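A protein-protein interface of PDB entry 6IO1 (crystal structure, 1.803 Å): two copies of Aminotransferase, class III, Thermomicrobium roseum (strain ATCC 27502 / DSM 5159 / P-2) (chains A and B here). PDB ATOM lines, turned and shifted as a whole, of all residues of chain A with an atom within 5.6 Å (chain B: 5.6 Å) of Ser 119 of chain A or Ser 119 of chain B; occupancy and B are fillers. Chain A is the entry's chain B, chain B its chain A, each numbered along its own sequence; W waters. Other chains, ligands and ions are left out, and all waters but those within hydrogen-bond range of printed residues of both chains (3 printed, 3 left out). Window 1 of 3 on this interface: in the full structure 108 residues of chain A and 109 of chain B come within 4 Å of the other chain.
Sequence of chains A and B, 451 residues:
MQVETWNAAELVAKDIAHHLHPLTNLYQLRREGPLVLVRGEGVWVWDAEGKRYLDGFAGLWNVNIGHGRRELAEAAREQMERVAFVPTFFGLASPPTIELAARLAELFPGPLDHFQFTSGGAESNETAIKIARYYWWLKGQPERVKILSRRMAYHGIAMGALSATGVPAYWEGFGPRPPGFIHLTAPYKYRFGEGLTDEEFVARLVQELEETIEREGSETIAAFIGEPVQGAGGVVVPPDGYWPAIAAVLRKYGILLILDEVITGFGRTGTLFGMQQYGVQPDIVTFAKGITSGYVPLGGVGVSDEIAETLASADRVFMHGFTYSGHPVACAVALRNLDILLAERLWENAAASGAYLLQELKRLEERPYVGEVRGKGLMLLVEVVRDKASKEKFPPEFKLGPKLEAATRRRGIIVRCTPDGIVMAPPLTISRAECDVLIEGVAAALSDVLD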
ATOM      1  N   PHE A 117       6.652 -19.096  -9.270  1.00  0.00           N
ATOM      2  CA  PHE A 117       6.422 -17.703  -9.615  1.00  0.00           C
ATOM      3  C   PHE A 117       7.691 -16.866  -9.477  1.00  0.00           C
ATOM      4  O   PHE A 117       8.662 -17.253  -8.824  1.00  0.00           O
ATOM      5  CB  PHE A 117       5.296 -17.135  -8.755  1.00  0.00           C
ATOM      6  CG  PHE A 117       3.984 -17.832  -8.964  1.00  0.00           C
ATOM      7  CD1 PHE A 117       3.274 -17.655 -10.140  1.00  0.00           C
ATOM      8  CD2 PHE A 117       3.474 -18.689  -8.002  1.00  0.00           C
ATOM      9  CE1 PHE A 117       2.074 -18.303 -10.347  1.00  0.00           C
ATOM     10  CE2 PHE A 117       2.272 -19.340  -8.204  1.00  0.00           C
ATOM     11  CZ  PHE A 117       1.570 -19.147  -9.378  1.00  0.00           C
ATOM     12  N   THR A 118       7.672 -15.714 -10.143  1.00  0.00           N
ATOM     13  CA  THR A 118       8.772 -14.761 -10.209  1.00  0.00           C
ATOM     14  C   THR A 118       8.159 -13.364 -10.200  1.00  0.00           C
ATOM     15  O   THR A 118       6.955 -13.196  -9.978  1.00  0.00           O
ATOM     16  CB  THR A 118       9.639 -14.971 -11.461  1.00  0.00           C
ATOM     17  OG1 THR A 118       8.868 -14.678 -12.633  1.00  0.00           O
ATOM     18  CG2 THR A 118      10.176 -16.396 -11.547  1.00  0.00           C
ATOM     19  N   SER A 119       8.989 -12.350 -10.438  1.00  0.00           N
ATOM     20  CA  SER A 119       8.521 -10.974 -10.508  1.00  0.00           C
ATOM     21  C   SER A 119       8.623 -10.359 -11.898  1.00  0.00           C
ATOM     22  O   SER A 119       8.249  -9.194 -12.067  1.00  0.00           O
ATOM     23  CB  SER A 119       9.291 -10.105  -9.508  1.00  0.00           C
ATOM     24  OG  SER A 119       8.995 -10.481  -8.176  1.00  0.00           O
ATOM     25  N   GLY A 120       9.101 -11.096 -12.897  1.00  0.00           N
ATOM     26  CA  GLY A 120       9.245 -10.506 -14.217  1.00  0.00           C
ATOM     27  C   GLY A 120       9.556 -11.543 -15.271  1.00  0.00           C
ATOM     28  O   GLY A 120       9.805 -12.714 -14.976  1.00  0.00           O
ATOM     29  N   GLY A 121       9.530 -11.081 -16.525  1.00  0.00           N
ATOM     30  CA  GLY A 121       9.782 -11.971 -17.647  1.00  0.00           C
ATOM     31  C   GLY A 121      11.197 -12.521 -17.679  1.00  0.00           C
ATOM     32  O   GLY A 121      11.404 -13.702 -17.964  1.00  0.00           O
ATOM     33  N   GLU A 123      13.240 -12.928 -15.136  1.00  0.00           N
ATOM     34  CA  GLU A 123      13.324 -13.917 -14.066  1.00  0.00           C
ATOM     35  C   GLU A 123      12.692 -15.233 -14.499  1.00  0.00           C
ATOM     36  O   GLU A 123      13.244 -16.311 -14.244  1.00  0.00           O
ATOM     37  CB  GLU A 123      12.636 -13.388 -12.808  1.00  0.00           C
ATOM     38  CG  GLU A 123      13.432 -12.366 -12.014  1.00  0.00           C
ATOM     39  CD  GLU A 123      12.759 -12.001 -10.701  1.00  0.00           C
ATOM     40  OE1 GLU A 123      11.687 -12.569 -10.403  1.00  0.00           O
ATOM     41  OE2 GLU A 123      13.299 -11.147  -9.967  1.00  0.00           O
ATOM     42  N   PRO A 297       4.013  -6.379  -9.868  1.00  0.00           N
ATOM     43  CA  PRO A 297       4.999  -7.210 -10.582  1.00  0.00           C
ATOM     44  C   PRO A 297       4.797  -8.689 -10.292  1.00  0.00           C
ATOM     45  O   PRO A 297       4.846  -9.128  -9.141  1.00  0.00           O
ATOM     46  CB  PRO A 297       6.340  -6.704 -10.041  1.00  0.00           C
ATOM     47  CG  PRO A 297       6.068  -5.299  -9.639  1.00  0.00           C
ATOM     48  CD  PRO A 297       4.662  -5.298  -9.105  1.00  0.00           C
ATOM     49  N   LEU A 298       4.563  -9.458 -11.353  1.00  0.00           N
ATOM     50  CA  LEU A 298       4.381 -10.895 -11.228  1.00  0.00           C
ATOM     51  C   LEU A 298       4.788 -11.579 -12.524  1.00  0.00           C
ATOM     52  O   LEU A 298       4.562 -11.053 -13.616  1.00  0.00           O
ATOM     53  CB  LEU A 298       2.931 -11.251 -10.879  1.00  0.00           C
ATOM     54  CG  LEU A 298       2.647 -12.738 -10.651  1.00  0.00           C
ATOM     55  CD1 LEU A 298       3.578 -13.309  -9.594  1.00  0.00           C
ATOM     56  CD2 LEU A 298       1.202 -12.962 -10.263  1.00  0.00           C
ATOM     57  N   GLY A 299       5.395 -12.755 -12.384  1.00  0.00           N
ATOM     58  CA  GLY A 299       5.787 -13.593 -13.495  1.00  0.00           C
ATOM     59  C   GLY A 299       5.736 -15.029 -13.027  1.00  0.00           C
ATOM     60  O   GLY A 299       5.461 -15.305 -11.859  1.00  0.00           O
ATOM     61  N   TYR A 324      11.041 -12.810  -4.120  1.00  0.00           N
ATOM     62  CA  TYR A 324       9.627 -12.467  -4.151  1.00  0.00           C
ATOM     63  C   TYR A 324       8.787 -13.478  -4.923  1.00  0.00           C
ATOM     64  O   TYR A 324       7.673 -13.149  -5.348  1.00  0.00           O
ATOM     65  CB  TYR A 324       9.451 -11.057  -4.715  1.00  0.00           C
ATOM     66  CG  TYR A 324       9.844 -10.009  -3.704  1.00  0.00           C
ATOM     67  CD1 TYR A 324       9.268  -9.997  -2.441  1.00  0.00           C
ATOM     68  CD2 TYR A 324      10.813  -9.057  -3.992  1.00  0.00           C
ATOM     69  CE1 TYR A 324       9.624  -9.056  -1.500  1.00  0.00           C
ATOM     70  CE2 TYR A 324      11.178  -8.108  -3.054  1.00  0.00           C
ATOM     71  CZ  TYR A 324      10.579  -8.114  -1.811  1.00  0.00           C
ATOM     72  OH  TYR A 324      10.932  -7.177  -0.869  1.00  0.00           O
ATOM     73  N   SER A 325       9.305 -14.687  -5.123  1.00  0.00           N
ATOM     74  CA  SER A 325       8.558 -15.740  -5.798  1.00  0.00           C
ATOM     75  C   SER A 325       7.255 -16.025  -5.061  1.00  0.00           C
ATOM     76  O   SER A 325       7.264 -16.355  -3.871  1.00  0.00           O
ATOM     77  CB  SER A 325       9.410 -17.005  -5.878  1.00  0.00           C
ATOM     78  OG  SER A 325       8.615 -18.137  -6.182  1.00  0.00           O
ATOM     79  N   PHE B 117      15.468   1.539 -10.794  1.00  0.00           N
ATOM     80  CA  PHE B 117      14.761   0.577  -9.966  1.00  0.00           C
ATOM     81  C   PHE B 117      14.581  -0.763 -10.674  1.00  0.00           C
ATOM     82  O   PHE B 117      14.693  -0.878 -11.896  1.00  0.00           O
ATOM     83  CB  PHE B 117      13.410   1.148  -9.538  1.00  0.00           C
ATOM     84  CG  PHE B 117      13.528   2.382  -8.693  1.00  0.00           C
ATOM     85  CD1 PHE B 117      13.994   2.300  -7.392  1.00  0.00           C
ATOM     86  CD2 PHE B 117      13.199   3.627  -9.205  1.00  0.00           C
ATOM     87  CE1 PHE B 117      14.117   3.431  -6.610  1.00  0.00           C
ATOM     88  CE2 PHE B 117      13.319   4.764  -8.427  1.00  0.00           C
ATOM     89  CZ  PHE B 117      13.778   4.665  -7.129  1.00  0.00           C
ATOM     90  N   THR B 118      14.323  -1.788  -9.864  1.00  0.00           N
ATOM     91  CA  THR B 118      14.153  -3.173 -10.281  1.00  0.00           C
ATOM     92  C   THR B 118      13.063  -3.778  -9.401  1.00  0.00           C
ATOM     93  O   THR B 118      12.402  -3.075  -8.629  1.00  0.00           O
ATOM     94  CB  THR B 118      15.460  -3.974 -10.162  1.00  0.00           C
ATOM     95  OG1 THR B 118      15.825  -4.092  -8.781  1.00  0.00           O
ATOM     96  CG2 THR B 118      16.600  -3.317 -10.934  1.00  0.00           C
ATOM     97  N   SER B 119      12.876  -5.092  -9.506  1.00  0.00           N
ATOM     98  CA  SER B 119      11.896  -5.794  -8.688  1.00  0.00           C
ATOM     99  C   SER B 119      12.515  -6.743  -7.670  1.00  0.00           C
ATOM    100  O   SER B 119      11.772  -7.392  -6.926  1.00  0.00           O
ATOM    101  CB  SER B 119      10.923  -6.569  -9.582  1.00  0.00           C
ATOM    102  OG  SER B 119      10.143  -5.688 -10.368  1.00  0.00           O
ATOM    103  N   GLY B 120      13.839  -6.843  -7.604  1.00  0.00           N
ATOM    104  CA  GLY B 120      14.441  -7.768  -6.660  1.00  0.00           C
ATOM    105  C   GLY B 120      15.935  -7.568  -6.551  1.00  0.00           C
ATOM    106  O   GLY B 120      16.548  -6.819  -7.316  1.00  0.00           O
ATOM    107  N   GLY B 121      16.514  -8.265  -5.569  1.00  0.00           N
ATOM    108  CA  GLY B 121      17.945  -8.157  -5.329  1.00  0.00           C
ATOM    109  C   GLY B 121      18.786  -8.693  -6.470  1.00  0.00           C
ATOM    110  O   GLY B 121      19.804  -8.099  -6.834  1.00  0.00           O
ATOM    111  N   GLU B 123      17.967  -8.906  -9.656  1.00  0.00           N
ATOM    112  CA  GLU B 123      17.884  -7.928 -10.735  1.00  0.00           C
ATOM    113  C   GLU B 123      18.794  -6.739 -10.459  1.00  0.00           C
ATOM    114  O   GLU B 123      19.480  -6.246 -11.363  1.00  0.00           O
ATOM    115  CB  GLU B 123      16.440  -7.460 -10.911  1.00  0.00           C
ATOM    116  CG  GLU B 123      15.524  -8.451 -11.611  1.00  0.00           C
ATOM    117  CD  GLU B 123      14.146  -7.874 -11.879  1.00  0.00           C
ATOM    118  OE1 GLU B 123      13.926  -6.684 -11.569  1.00  0.00           O
ATOM    119  OE2 GLU B 123      13.280  -8.610 -12.398  1.00  0.00           O
ATOM    120  N   PRO B 297       7.138  -6.096  -4.320  1.00  0.00           N
ATOM    121  CA  PRO B 297       8.493  -6.339  -4.843  1.00  0.00           C
ATOM    122  C   PRO B 297       9.122  -5.061  -5.374  1.00  0.00           C
ATOM    123  O   PRO B 297       8.584  -4.407  -6.272  1.00  0.00           O
ATOM    124  CB  PRO B 297       8.257  -7.362  -5.960  1.00  0.00           C
ATOM    125  CG  PRO B 297       7.013  -8.068  -5.554  1.00  0.00           C
ATOM    126  CD  PRO B 297       6.152  -7.024  -4.902  1.00  0.00           C
ATOM    127  N   LEU B 298      10.271  -4.704  -4.806  1.00  0.00           N
ATOM    128  CA  LEU B 298      11.000  -3.521  -5.236  1.00  0.00           C
ATOM    129  C   LEU B 298      12.482  -3.703  -4.951  1.00  0.00           C
ATOM    130  O   LEU B 298      12.864  -4.284  -3.932  1.00  0.00           O
ATOM    131  CB  LEU B 298      10.483  -2.256  -4.541  1.00  0.00           C
ATOM    132  CG  LEU B 298      11.153  -0.942  -4.951  1.00  0.00           C
ATOM    133  CD1 LEU B 298      11.073  -0.747  -6.455  1.00  0.00           C
ATOM    134  CD2 LEU B 298      10.532   0.234  -4.227  1.00  0.00           C
ATOM    135  N   GLY B 299      13.308  -3.200  -5.865  1.00  0.00           N
ATOM    136  CA  GLY B 299      14.748  -3.212  -5.731  1.00  0.00           C
ATOM    137  C   GLY B 299      15.295  -2.012  -6.470  1.00  0.00           C
ATOM    138  O   GLY B 299      14.549  -1.260  -7.096  1.00  0.00           O
ATOM    139  N   TYR B 324       9.257  -3.896 -15.029  1.00  0.00           N
ATOM    140  CA  TYR B 324       8.612  -3.277 -13.882  1.00  0.00           C
ATOM    141  C   TYR B 324       9.521  -2.306 -13.138  1.00  0.00           C
ATOM    142  O   TYR B 324       9.254  -1.989 -11.973  1.00  0.00           O
ATOM    143  CB  TYR B 324       8.075  -4.361 -12.948  1.00  0.00           C
ATOM    144  CG  TYR B 324       6.874  -5.044 -13.550  1.00  0.00           C
ATOM    145  CD1 TYR B 324       5.804  -4.296 -14.021  1.00  0.00           C
ATOM    146  CD2 TYR B 324       6.820  -6.424 -13.687  1.00  0.00           C
ATOM    147  CE1 TYR B 324       4.707  -4.898 -14.592  1.00  0.00           C
ATOM    148  CE2 TYR B 324       5.719  -7.039 -14.256  1.00  0.00           C
ATOM    149  CZ  TYR B 324       4.666  -6.269 -14.704  1.00  0.00           C
ATOM    150  OH  TYR B 324       3.565  -6.865 -15.272  1.00  0.00           O
ATOM    151  N   SER B 325      10.591  -1.845 -13.781  1.00  0.00           N
ATOM    152  CA  SER B 325      11.485  -0.863 -13.179  1.00  0.00           C
ATOM    153  C   SER B 325      10.716   0.400 -12.815  1.00  0.00           C
ATOM    154  O   SER B 325      10.083   1.021 -13.674  1.00  0.00           O
ATOM    155  CB  SER B 325      12.621  -0.533 -14.146  1.00  0.00           C
ATOM    156  OG  SER B 325      13.264   0.675 -13.782  1.00  0.00           O
HETATM  157  O   HOH W   1      10.629  -7.684 -12.567  1.00  0.00           O
HETATM  158  O   HOH W   2      15.538 -10.131  -8.581  1.00  0.00           O
HETATM  159  O   HOH W   3      12.508 -10.124 -14.501  1.00  0.00           O
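Ser 119 of chain A touches Ser 119 of chain B (CB to CB, 3.9 Å). OG of Ser 119 of chain A touches CB of Pro 297 of chain B, at 3.9 Å. O of Ser 119 of chain A touches CD2 of Tyr 324 of chain B (3.5 Å). Glu 123 of chain A touches Glu 123 of chain B. Pro 297 of chain A touches Ser 119 of chain B. Tyr 324 of chain B touches Pro 297 of chain A (CD2 to CA, 3.7 Å). Leu 298 of chain A touches Tyr 324 of chain B. Tyr 324 of chain A touches Ser 119 of chain B (CD2 to O, 3.5 Å). Tyr 324 of chain A touches Pro 297 of chain B (CD2 to CB, 3.6 Å). N of Leu 298 of chain B touches CE2 of Tyr 324 of chain A (3.9 Å).
Of the 11 printed residues of chain A, 5 touch a printed residue of chain B. Hydrophobic or aromatic side chains of chain A within 4 Å of the printed part of chain B: Pro 297 and Tyr 324. Of the 11 printed residues of chain B, 5 touch a printed residue of chain A. Hydrophobic or aromatic side chains of chain B that line the printed part of chain A: Pro 297 and Tyr 324. Along chain B the printed residues that touch a printed residue of chain A span positions 119 to 324. Among the printed residues, no Asp or Glu carboxylate lies within 4 Å of a Lys or Arg side-chain nitrogen of the other chain.
Ser 119 of chain B touches three residues of chain A. Of the printed residues of chain A, Leu 298 of chain B touches Tyr 324 (3.9 Å). Of the printed residues of chain A, Glu 123 of chain B touches Glu 123 (3.5 Å). Gly 120 of chain B touches none of the printed residues of chain A. The nearest residue of chain B that does not touch Ser 119 of chain A is Glu 123 of chain B (5.0 Å).
Water W3 bridges OE2 of Glu 123 of chain B (2.7 Å) and N of Glu 123 of chain A (3.0 Å). Water W1 lies within hydrogen-bond range of OE2 of Glu 123 of chain B, O of Ser 119 of chain A and OG of Ser 119 of chain B. Water W2 lies within hydrogen-bond range of OE2 of Glu 123 of chain A (2.8 Å) and N of Glu 123 of chain B (2.9 Å).
The side-chain carboxylate of Glu 123 of chain B lies within hydrogen-bond range of the backbone NH of Ser 119 of chain B, 2.8 Å away. The backbone NH (N) of Ser 119 of chain A lies within hydrogen-bond range of the side-chain carboxylate (OE1) of Glu 123 of chain A, 2.7 Å away.
Ser 119 of chain A touches its own counterpart, Ser 119 of chain B. Ser 119 of chain A touches Tyr 324 of chain B, and with the chains exchanged Tyr 324 of chain A touches Ser 119 of chain B. Glu 123 of chain A touches its own counterpart, Glu 123 of chain B. Leu 298 of chain A touches Tyr 324 of chain B, and with the chains exchanged Tyr 324 of chain A touches Leu 298 of chain B.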
